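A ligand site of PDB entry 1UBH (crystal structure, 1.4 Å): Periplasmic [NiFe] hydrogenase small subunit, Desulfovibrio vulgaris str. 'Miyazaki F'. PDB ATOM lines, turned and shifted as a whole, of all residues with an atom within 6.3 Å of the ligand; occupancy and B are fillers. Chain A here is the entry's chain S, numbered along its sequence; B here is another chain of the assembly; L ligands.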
ATOM      1  N   ALA A  15      15.095  -4.749  -1.955  1.00  0.00           N
ATOM      2  CA  ALA A  15      16.088  -4.003  -2.706  1.00  0.00           C
ATOM      3  C   ALA A  15      17.309  -3.944  -1.804  1.00  0.00           C
ATOM      4  O   ALA A  15      17.373  -3.167  -0.864  1.00  0.00           O
ATOM      5  CB  ALA A  15      15.576  -2.621  -3.098  1.00  0.00           C
ATOM      6  N   GLU A  16      18.267  -4.813  -2.083  1.00  0.00           N
ATOM      7  CA  GLU A  16      19.369  -5.048  -1.168  1.00  0.00           C
ATOM      8  C   GLU A  16      20.619  -5.463  -1.903  1.00  0.00           C
ATOM      9  O   GLU A  16      20.540  -5.835  -3.065  1.00  0.00           O
ATOM     10  CB  GLU A  16      18.958  -6.112  -0.115  1.00  0.00           C
ATOM     11  CG  GLU A  16      18.228  -7.336  -0.661  1.00  0.00           C
ATOM     12  CD  GLU A  16      19.115  -8.430  -1.241  1.00  0.00           C
ATOM     13  OE1 GLU A  16      20.229  -8.692  -0.667  1.00  0.00           O
ATOM     14  OE2 GLU A  16      18.716  -9.079  -2.234  1.00  0.00           O
ATOM     15  N   CYS A  17      21.767  -5.393  -1.217  1.00  0.00           N
ATOM     16  CA  CYS A  17      23.030  -5.791  -1.820  1.00  0.00           C
ATOM     17  C   CYS A  17      23.537  -7.120  -1.266  1.00  0.00           C
ATOM     18  O   CYS A  17      24.584  -7.584  -1.715  1.00  0.00           O
ATOM     19  CB  CYS A  17      24.060  -4.707  -1.556  1.00  0.00           C
ATOM     20  SG  CYS A  17      24.807  -4.755   0.104  1.00  0.00           S
ATOM     21  N   THR A  18      22.840  -7.684  -0.308  1.00  0.00           N
ATOM     22  CA  THR A  18      23.121  -8.989   0.293  1.00  0.00           C
ATOM     23  C   THR A  18      24.253  -8.857   1.308  1.00  0.00           C
ATOM     24  O   THR A  18      24.655  -9.848   1.910  1.00  0.00           O
ATOM     25  CB  THR A  18      23.323 -10.071  -0.772  1.00  0.00           C
ATOM     26  OG1 THR A  18      22.222  -9.997  -1.713  1.00  0.00           O
ATOM     27  CG2 THR A  18      23.269 -11.487  -0.234  1.00  0.00           C
ATOM     28  N   GLY A  19      24.745  -7.674   1.553  1.00  0.00           N
ATOM     29  CA  GLY A  19      25.705  -7.396   2.633  1.00  0.00           C
ATOM     30  C   GLY A  19      25.116  -7.691   4.003  1.00  0.00           C
ATOM     31  O   GLY A  19      25.827  -8.165   4.903  1.00  0.00           O
ATOM     32  N   CYS A  20      23.827  -7.452   4.185  1.00  0.00           N
ATOM     33  CA  CYS A  20      23.197  -7.818   5.454  1.00  0.00           C
ATOM     34  C   CYS A  20      23.164  -9.323   5.610  1.00  0.00           C
ATOM     35  O   CYS A  20      23.498  -9.845   6.691  1.00  0.00           O
ATOM     36  CB  CYS A  20      21.831  -7.114   5.585  1.00  0.00           C
ATOM     37  SG  CYS A  20      21.953  -5.372   5.874  1.00  0.00           S
ATOM     38  N   SER A  21      22.786 -10.069   4.566  1.00  0.00           N
ATOM     39  CA  SER A  21      22.824 -11.524   4.650  1.00  0.00           C
ATOM     40  C   SER A  21      24.227 -12.019   5.017  1.00  0.00           C
ATOM     41  O   SER A  21      24.391 -12.896   5.868  1.00  0.00           O
ATOM     42  CB  SER A  21      22.423 -12.190   3.343  1.00  0.00           C
ATOM     43  OG  SER A  21      21.023 -12.162   3.166  1.00  0.00           O
ATOM     44  N   GLU A  75      15.597  -7.916   4.816  1.00  0.00           N
ATOM     45  CA  GLU A  75      16.739  -7.195   4.285  1.00  0.00           C
ATOM     46  C   GLU A  75      16.362  -6.406   3.054  1.00  0.00           C
ATOM     47  O   GLU A  75      15.676  -6.968   2.202  1.00  0.00           O
ATOM     48  CB  GLU A  75      17.867  -8.220   3.998  1.00  0.00           C
ATOM     49  CG  GLU A  75      19.081  -7.701   3.263  1.00  0.00           C
ATOM     50  CD  GLU A  75      20.216  -8.692   3.133  1.00  0.00           C
ATOM     51  OE1 GLU A  75      21.296  -8.322   2.657  1.00  0.00           O
ATOM     52  OE2 GLU A  75      19.924  -9.853   3.539  1.00  0.00           O
ATOM     53  N   GLY A  76      16.701  -5.122   2.912  1.00  0.00           N
ATOM     54  CA  GLY A  76      16.464  -4.342   1.736  1.00  0.00           C
ATOM     55  C   GLY A  76      15.252  -3.418   1.869  1.00  0.00           C
ATOM     56  O   GLY A  76      14.290  -3.659   2.606  1.00  0.00           O
ATOM     57  N   GLY A  77      15.318  -2.310   1.134  1.00  0.00           N
ATOM     58  CA  GLY A  77      14.226  -1.385   1.011  1.00  0.00           C
ATOM     59  C   GLY A  77      13.123  -1.866   0.102  1.00  0.00           C
ATOM     60  O   GLY A  77      13.343  -2.771  -0.699  1.00  0.00           O
ATOM     61  N   TYR A 111      16.349  -5.537   9.103  1.00  0.00           N
ATOM     62  CA  TYR A 111      17.758  -5.756   9.338  1.00  0.00           C
ATOM     63  C   TYR A 111      18.530  -5.026   8.233  1.00  0.00           C
ATOM     64  O   TYR A 111      18.429  -5.346   7.042  1.00  0.00           O
ATOM     65  CB  TYR A 111      18.105  -7.253   9.391  1.00  0.00           C
ATOM     66  CG  TYR A 111      19.550  -7.528   9.731  1.00  0.00           C
ATOM     67  CD1 TYR A 111      20.057  -7.110  10.968  1.00  0.00           C
ATOM     68  CD2 TYR A 111      20.437  -8.142   8.870  1.00  0.00           C
ATOM     69  CE1 TYR A 111      21.372  -7.326  11.330  1.00  0.00           C
ATOM     70  CE2 TYR A 111      21.751  -8.364   9.214  1.00  0.00           C
ATOM     71  CZ  TYR A 111      22.230  -7.951  10.431  1.00  0.00           C
ATOM     72  OH  TYR A 111      23.532  -8.142  10.817  1.00  0.00           O
ATOM     73  N   GLY A 112      19.288  -4.000   8.660  1.00  0.00           N
ATOM     74  CA  GLY A 112      20.093  -3.143   7.870  1.00  0.00           C
ATOM     75  C   GLY A 112      19.365  -1.845   7.585  1.00  0.00           C
ATOM     76  O   GLY A 112      18.128  -1.800   7.518  1.00  0.00           O
ATOM     77  N   THR A 113      20.133  -0.781   7.391  1.00  0.00           N
ATOM     78  CA  THR A 113      19.620   0.537   7.054  1.00  0.00           C
ATOM     79  C   THR A 113      18.676   0.575   5.890  1.00  0.00           C
ATOM     80  O   THR A 113      17.772   1.409   5.861  1.00  0.00           O
ATOM     81  CB  THR A 113      20.799   1.499   6.796  1.00  0.00           C
ATOM     82  OG1 THR A 113      21.438   1.644   8.025  1.00  0.00           O
ATOM     83  CG2 THR A 113      20.352   2.908   6.436  1.00  0.00           C
ATOM     84  N   CYS A 114      18.882  -0.230   4.861  1.00  0.00           N
ATOM     85  CA  CYS A 114      17.904  -0.239   3.768  1.00  0.00           C
ATOM     86  C   CYS A 114      16.520  -0.665   4.258  1.00  0.00           C
ATOM     87  O   CYS A 114      15.538   0.044   4.031  1.00  0.00           O
ATOM     88  CB  CYS A 114      18.295  -1.136   2.643  1.00  0.00           C
ATOM     89  SG  CYS A 114      19.916  -0.768   1.831  1.00  0.00           S
ATOM     90  N   ALA A 115      16.421  -1.828   4.917  1.00  0.00           N
ATOM     91  CA  ALA A 115      15.171  -2.241   5.497  1.00  0.00           C
ATOM     92  C   ALA A 115      14.627  -1.318   6.571  1.00  0.00           C
ATOM     93  O   ALA A 115      13.391  -1.145   6.670  1.00  0.00           O
ATOM     94  CB  ALA A 115      15.287  -3.635   6.100  1.00  0.00           C
ATOM     95  N   GLY A 119      17.691   3.250   2.934  1.00  0.00           N
ATOM     96  CA  GLY A 119      19.052   2.952   2.485  1.00  0.00           C
ATOM     97  C   GLY A 119      19.506   3.490   1.166  1.00  0.00           C
ATOM     98  O   GLY A 119      19.011   4.498   0.686  1.00  0.00           O
ATOM     99  N   VAL A 120      20.479   2.794   0.558  1.00  0.00           N
ATOM    100  CA  VAL A 120      21.223   3.375  -0.546  1.00  0.00           C
ATOM    101  C   VAL A 120      20.332   3.672  -1.731  1.00  0.00           C
ATOM    102  O   VAL A 120      20.470   4.739  -2.334  1.00  0.00           O
ATOM    103  CB  VAL A 120      22.422   2.480  -0.914  1.00  0.00           C
ATOM    104  CG1 VAL A 120      22.045   1.202  -1.593  1.00  0.00           C
ATOM    105  CG2 VAL A 120      23.417   3.306  -1.758  1.00  0.00           C
ATOM    106  N   GLN A 121      19.388   2.808  -2.054  1.00  0.00           N
ATOM    107  CA  GLN A 121      18.536   3.081  -3.209  1.00  0.00           C
ATOM    108  C   GLN A 121      17.507   4.185  -2.909  1.00  0.00           C
ATOM    109  O   GLN A 121      16.911   4.749  -3.843  1.00  0.00           O
ATOM    110  CB  GLN A 121      17.824   1.836  -3.705  1.00  0.00           C
ATOM    111  CG  GLN A 121      16.994   1.077  -2.696  1.00  0.00           C
ATOM    112  CD  GLN A 121      17.865   0.145  -1.886  1.00  0.00           C
ATOM    113  OE1 GLN A 121      18.683  -0.606  -2.419  1.00  0.00           O
ATOM    114  NE2 GLN A 121      17.666   0.142  -0.584  1.00  0.00           N
ATOM    115  N   GLY A 149      22.465  -0.146  10.498  1.00  0.00           N
ATOM    116  CA  GLY A 149      23.790  -0.234   9.952  1.00  0.00           C
ATOM    117  C   GLY A 149      23.874  -0.754   8.512  1.00  0.00           C
ATOM    118  O   GLY A 149      22.932  -1.393   8.042  1.00  0.00           O
ATOM    119  N   CYS A 150      25.018  -0.593   7.876  1.00  0.00           N
ATOM    120  CA  CYS A 150      25.176  -0.912   6.468  1.00  0.00           C
ATOM    121  C   CYS A 150      26.433  -1.695   6.155  1.00  0.00           C
ATOM    122  O   CYS A 150      27.387  -1.205   5.519  1.00  0.00           O
ATOM    123  CB  CYS A 150      25.113   0.392   5.674  1.00  0.00           C
ATOM    124  SG  CYS A 150      24.847   0.238   3.923  1.00  0.00           S
ATOM    125  N   PRO A 151      26.472  -2.976   6.569  1.00  0.00           N
ATOM    126  CA  PRO A 151      25.442  -3.652   7.338  1.00  0.00           C
ATOM    127  C   PRO A 151      25.585  -3.514   8.850  1.00  0.00           C
ATOM    128  O   PRO A 151      26.599  -3.005   9.356  1.00  0.00           O
ATOM    129  CB  PRO A 151      25.708  -5.119   6.976  1.00  0.00           C
ATOM    130  CG  PRO A 151      27.204  -5.168   6.892  1.00  0.00           C
ATOM    131  CD  PRO A 151      27.577  -3.880   6.216  1.00  0.00           C
ATOM    132  N   PRO A 152      24.566  -3.920   9.574  1.00  0.00           N
ATOM    133  CA  PRO A 152      24.609  -3.869  11.045  1.00  0.00           C
ATOM    134  C   PRO A 152      25.645  -4.855  11.564  1.00  0.00           C
ATOM    135  O   PRO A 152      26.083  -5.759  10.846  1.00  0.00           O
ATOM    136  CB  PRO A 152      23.208  -4.250  11.508  1.00  0.00           C
ATOM    137  CG  PRO A 152      22.361  -4.175  10.287  1.00  0.00           C
ATOM    138  CD  PRO A 152      23.289  -4.488   9.124  1.00  0.00           C
ATOM    139  N   TRP A 258      22.979   8.641   3.549  1.00  0.00           N
ATOM    140  CA  TRP A 258      23.555   8.871   2.225  1.00  0.00           C
ATOM    141  C   TRP A 258      23.448  10.356   1.854  1.00  0.00           C
ATOM    142  O   TRP A 258      24.325  10.853   1.152  1.00  0.00           O
ATOM    143  CB  TRP A 258      22.879   7.971   1.176  1.00  0.00           C
ATOM    144  CG  TRP A 258      23.104   6.525   1.478  1.00  0.00           C
ATOM    145  CD1 TRP A 258      22.182   5.649   1.999  1.00  0.00           C
ATOM    146  CD2 TRP A 258      24.298   5.796   1.316  1.00  0.00           C
ATOM    147  NE1 TRP A 258      22.742   4.418   2.155  1.00  0.00           N
ATOM    148  CE2 TRP A 258      24.049   4.470   1.738  1.00  0.00           C
ATOM    149  CE3 TRP A 258      25.568   6.138   0.837  1.00  0.00           C
ATOM    150  CZ2 TRP A 258      25.046   3.473   1.698  1.00  0.00           C
ATOM    151  CZ3 TRP A 258      26.530   5.140   0.807  1.00  0.00           C
ATOM    152  CH2 TRP A 258      26.268   3.833   1.234  1.00  0.00           C
ATOM    153  N   ARG B  41      17.960  -0.722  -8.756  1.00  0.00           N
ATOM    154  CA  ARG B  41      18.170   0.290  -7.712  1.00  0.00           C
ATOM    155  C   ARG B  41      18.582   1.636  -8.282  1.00  0.00           C
ATOM    156  O   ARG B  41      18.151   2.654  -7.765  1.00  0.00           O
ATOM    157  CB  ARG B  41      19.208  -0.239  -6.689  1.00  0.00           C
ATOM    158  CG  ARG B  41      18.651  -1.319  -5.821  1.00  0.00           C
ATOM    159  CD  ARG B  41      19.615  -1.966  -4.871  1.00  0.00           C
ATOM    160  NE  ARG B  41      20.739  -2.530  -5.636  1.00  0.00           N
ATOM    161  CZ  ARG B  41      21.984  -2.727  -5.279  1.00  0.00           C
ATOM    162  NH1 ARG B  41      22.423  -2.447  -4.066  1.00  0.00           N
ATOM    163  NH2 ARG B  41      22.861  -3.216  -6.154  1.00  0.00           N
ATOM    164  N   ARG B  61      28.084  -0.516  -2.000  1.00  0.00           N
ATOM    165  CA  ARG B  61      26.742  -1.078  -1.727  1.00  0.00           C
ATOM    166  C   ARG B  61      26.057  -1.577  -2.986  1.00  0.00           C
ATOM    167  O   ARG B  61      24.889  -1.986  -2.909  1.00  0.00           O
ATOM    168  CB  ARG B  61      25.853  -0.051  -1.018  1.00  0.00           C
ATOM    169  CG  ARG B  61      26.105   0.038   0.470  1.00  0.00           C
ATOM    170  CD  ARG B  61      27.495   0.491   0.822  1.00  0.00           C
ATOM    171  NE  ARG B  61      27.701   0.533   2.252  1.00  0.00           N
ATOM    172  CZ  ARG B  61      28.791   0.959   2.883  1.00  0.00           C
ATOM    173  NH1 ARG B  61      29.816   1.445   2.173  1.00  0.00           N
ATOM    174  NH2 ARG B  61      28.863   0.898   4.203  1.00  0.00           N
ATOM    175  N   GLY B  64      27.214  -6.792  -1.468  1.00  0.00           N
ATOM    176  CA  GLY B  64      27.815  -7.229  -0.229  1.00  0.00           C
ATOM    177  C   GLY B  64      28.387  -8.610  -0.253  1.00  0.00           C
ATOM    178  O   GLY B  64      29.023  -9.023   0.732  1.00  0.00           O
ATOM    179  N   PRO B 216      31.079  -7.476   6.277  1.00  0.00           N
ATOM    180  CA  PRO B 216      31.077  -6.789   4.993  1.00  0.00           C
ATOM    181  C   PRO B 216      31.252  -5.290   5.126  1.00  0.00           C
ATOM    182  O   PRO B 216      31.039  -4.579   6.104  1.00  0.00           O
ATOM    183  CB  PRO B 216      29.692  -7.098   4.376  1.00  0.00           C
ATOM    184  CG  PRO B 216      29.208  -8.248   5.173  1.00  0.00           C
ATOM    185  CD  PRO B 216      29.752  -8.026   6.545  1.00  0.00           C
ATOM    186  N   HIS B 217      31.754  -4.703   4.097  1.00  0.00           N
ATOM    187  CA  HIS B 217      31.829  -3.383   3.508  1.00  0.00           C
ATOM    188  C   HIS B 217      32.995  -2.726   4.214  1.00  0.00           C
ATOM    189  O   HIS B 217      32.859  -2.091   5.251  1.00  0.00           O
ATOM    190  CB  HIS B 217      30.480  -2.641   3.625  1.00  0.00           C
ATOM    191  CG  HIS B 217      29.507  -3.065   2.555  1.00  0.00           C
ATOM    192  ND1 HIS B 217      28.170  -2.857   2.536  1.00  0.00           N
ATOM    193  CD2 HIS B 217      29.764  -3.729   1.368  1.00  0.00           C
ATOM    194  CE1 HIS B 217      27.651  -3.363   1.428  1.00  0.00           C
ATOM    195  NE2 HIS B 217      28.649  -3.902   0.698  1.00  0.00           N
HETATM  196 FE1  LIG L   1      23.467  -3.656   1.590  1.00  0.00          FE
HETATM  197 FE2  LIG L   1      21.383  -2.234   2.414  1.00  0.00          FE
HETATM  198 FE3  LIG L   1      23.764  -1.727   3.407  1.00  0.00          FE
HETATM  199 FE4  LIG L   1      22.508  -4.067   4.093  1.00  0.00          FE
HETATM  200  S1  LIG L   1      21.826  -1.965   4.675  1.00  0.00           S
HETATM  201  S2  LIG L   1      24.655  -3.704   3.554  1.00  0.00           S
HETATM  202  S3  LIG L   1      21.355  -4.497   2.133  1.00  0.00           S
HETATM  203  S4  LIG L   1      23.161  -1.483   1.163  1.00  0.00           S
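The side-chain sulfur (SG) of Cys 20 is bound to an iron atom (FE4) of the ligand (2.3 Å). FE2 of the ligand is bound by SG of Cys 114 (2.2 Å). N of Cys 17 lies close to S3 of the ligand (3.5 Å). The side-chain sulfur of Cys 150 is bound to an iron atom (FE3) of the ligand (2.3 Å). S1 of the ligand sits close to N of Thr 113 (3.4 Å). SG of Cys 17 is bound to FE1 of the ligand. The backbone NH of Cys 114 sits close to a sulfur (S1) of the ligand (3.4 Å). A ring nitrogen (ND1) of His 217 of chain B sits close to a sulfur (S2) of the ligand (3.8 Å).
The backbone carbonyl oxygen (O) of Cys 150 lies within hydrogen-bond range of a ring nitrogen (ND1) of His 217 of chain B, 3.5 Å away. The backbone carbonyl oxygen of Cys 150 sits at hydrogen-bond distance from the guanidinium group of Arg 61 of chain B. The side-chain hydroxyl (OG1) of Thr 18 is in hydrogen-bond range of the side-chain carboxylate (OE1) of Glu 16 (2.6 Å). OE2 of Glu 75 sits at hydrogen-bond distance from OG of Ser 21, at 2.6 Å. SG of Cys 114 lies close to NE2 of Gln 121 (3.4 Å). The backbone carbonyl oxygen (O) of Cys 17 sits at hydrogen-bond distance from the backbone NH (N) of Gly 64 of chain B (2.8 Å). The side-chain sulfur of Cys 20 lies close to the backbone carbonyl oxygen of Tyr 111, 3.7 Å away. The side-chain carboxylate of Glu 75 sits close to the backbone NH of Thr 18, 3.4 Å away.
The backbone carbonyl oxygen of Gly 149 sits close to a sulfur (S1) of the ligand (3.6 Å). The backbone nitrogen (N) of Pro 151 sits close to a sulfur (S2) of the ligand. CB of Glu 16 touches S3 of the ligand, 3.7 Å away. Gly 19 touches the ligand. Glu 75 touches the ligand. Gly 112 touches the ligand. Arg 61 of chain B touches the ligand (CG to S4, 3.4 Å). Hydrophobic or aromatic side chains within 4 Å of the ligand: Pro 151 and His 217 of chain B. Within 4 Å of the ligand: Glu 16, Cys 17, Gly 19, Cys 20, Glu 75, Gly 112, Thr 113, Cys 114, Gly 149, Cys 150, Pro 151, Arg 61 of chain B and His 217 of chain B.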
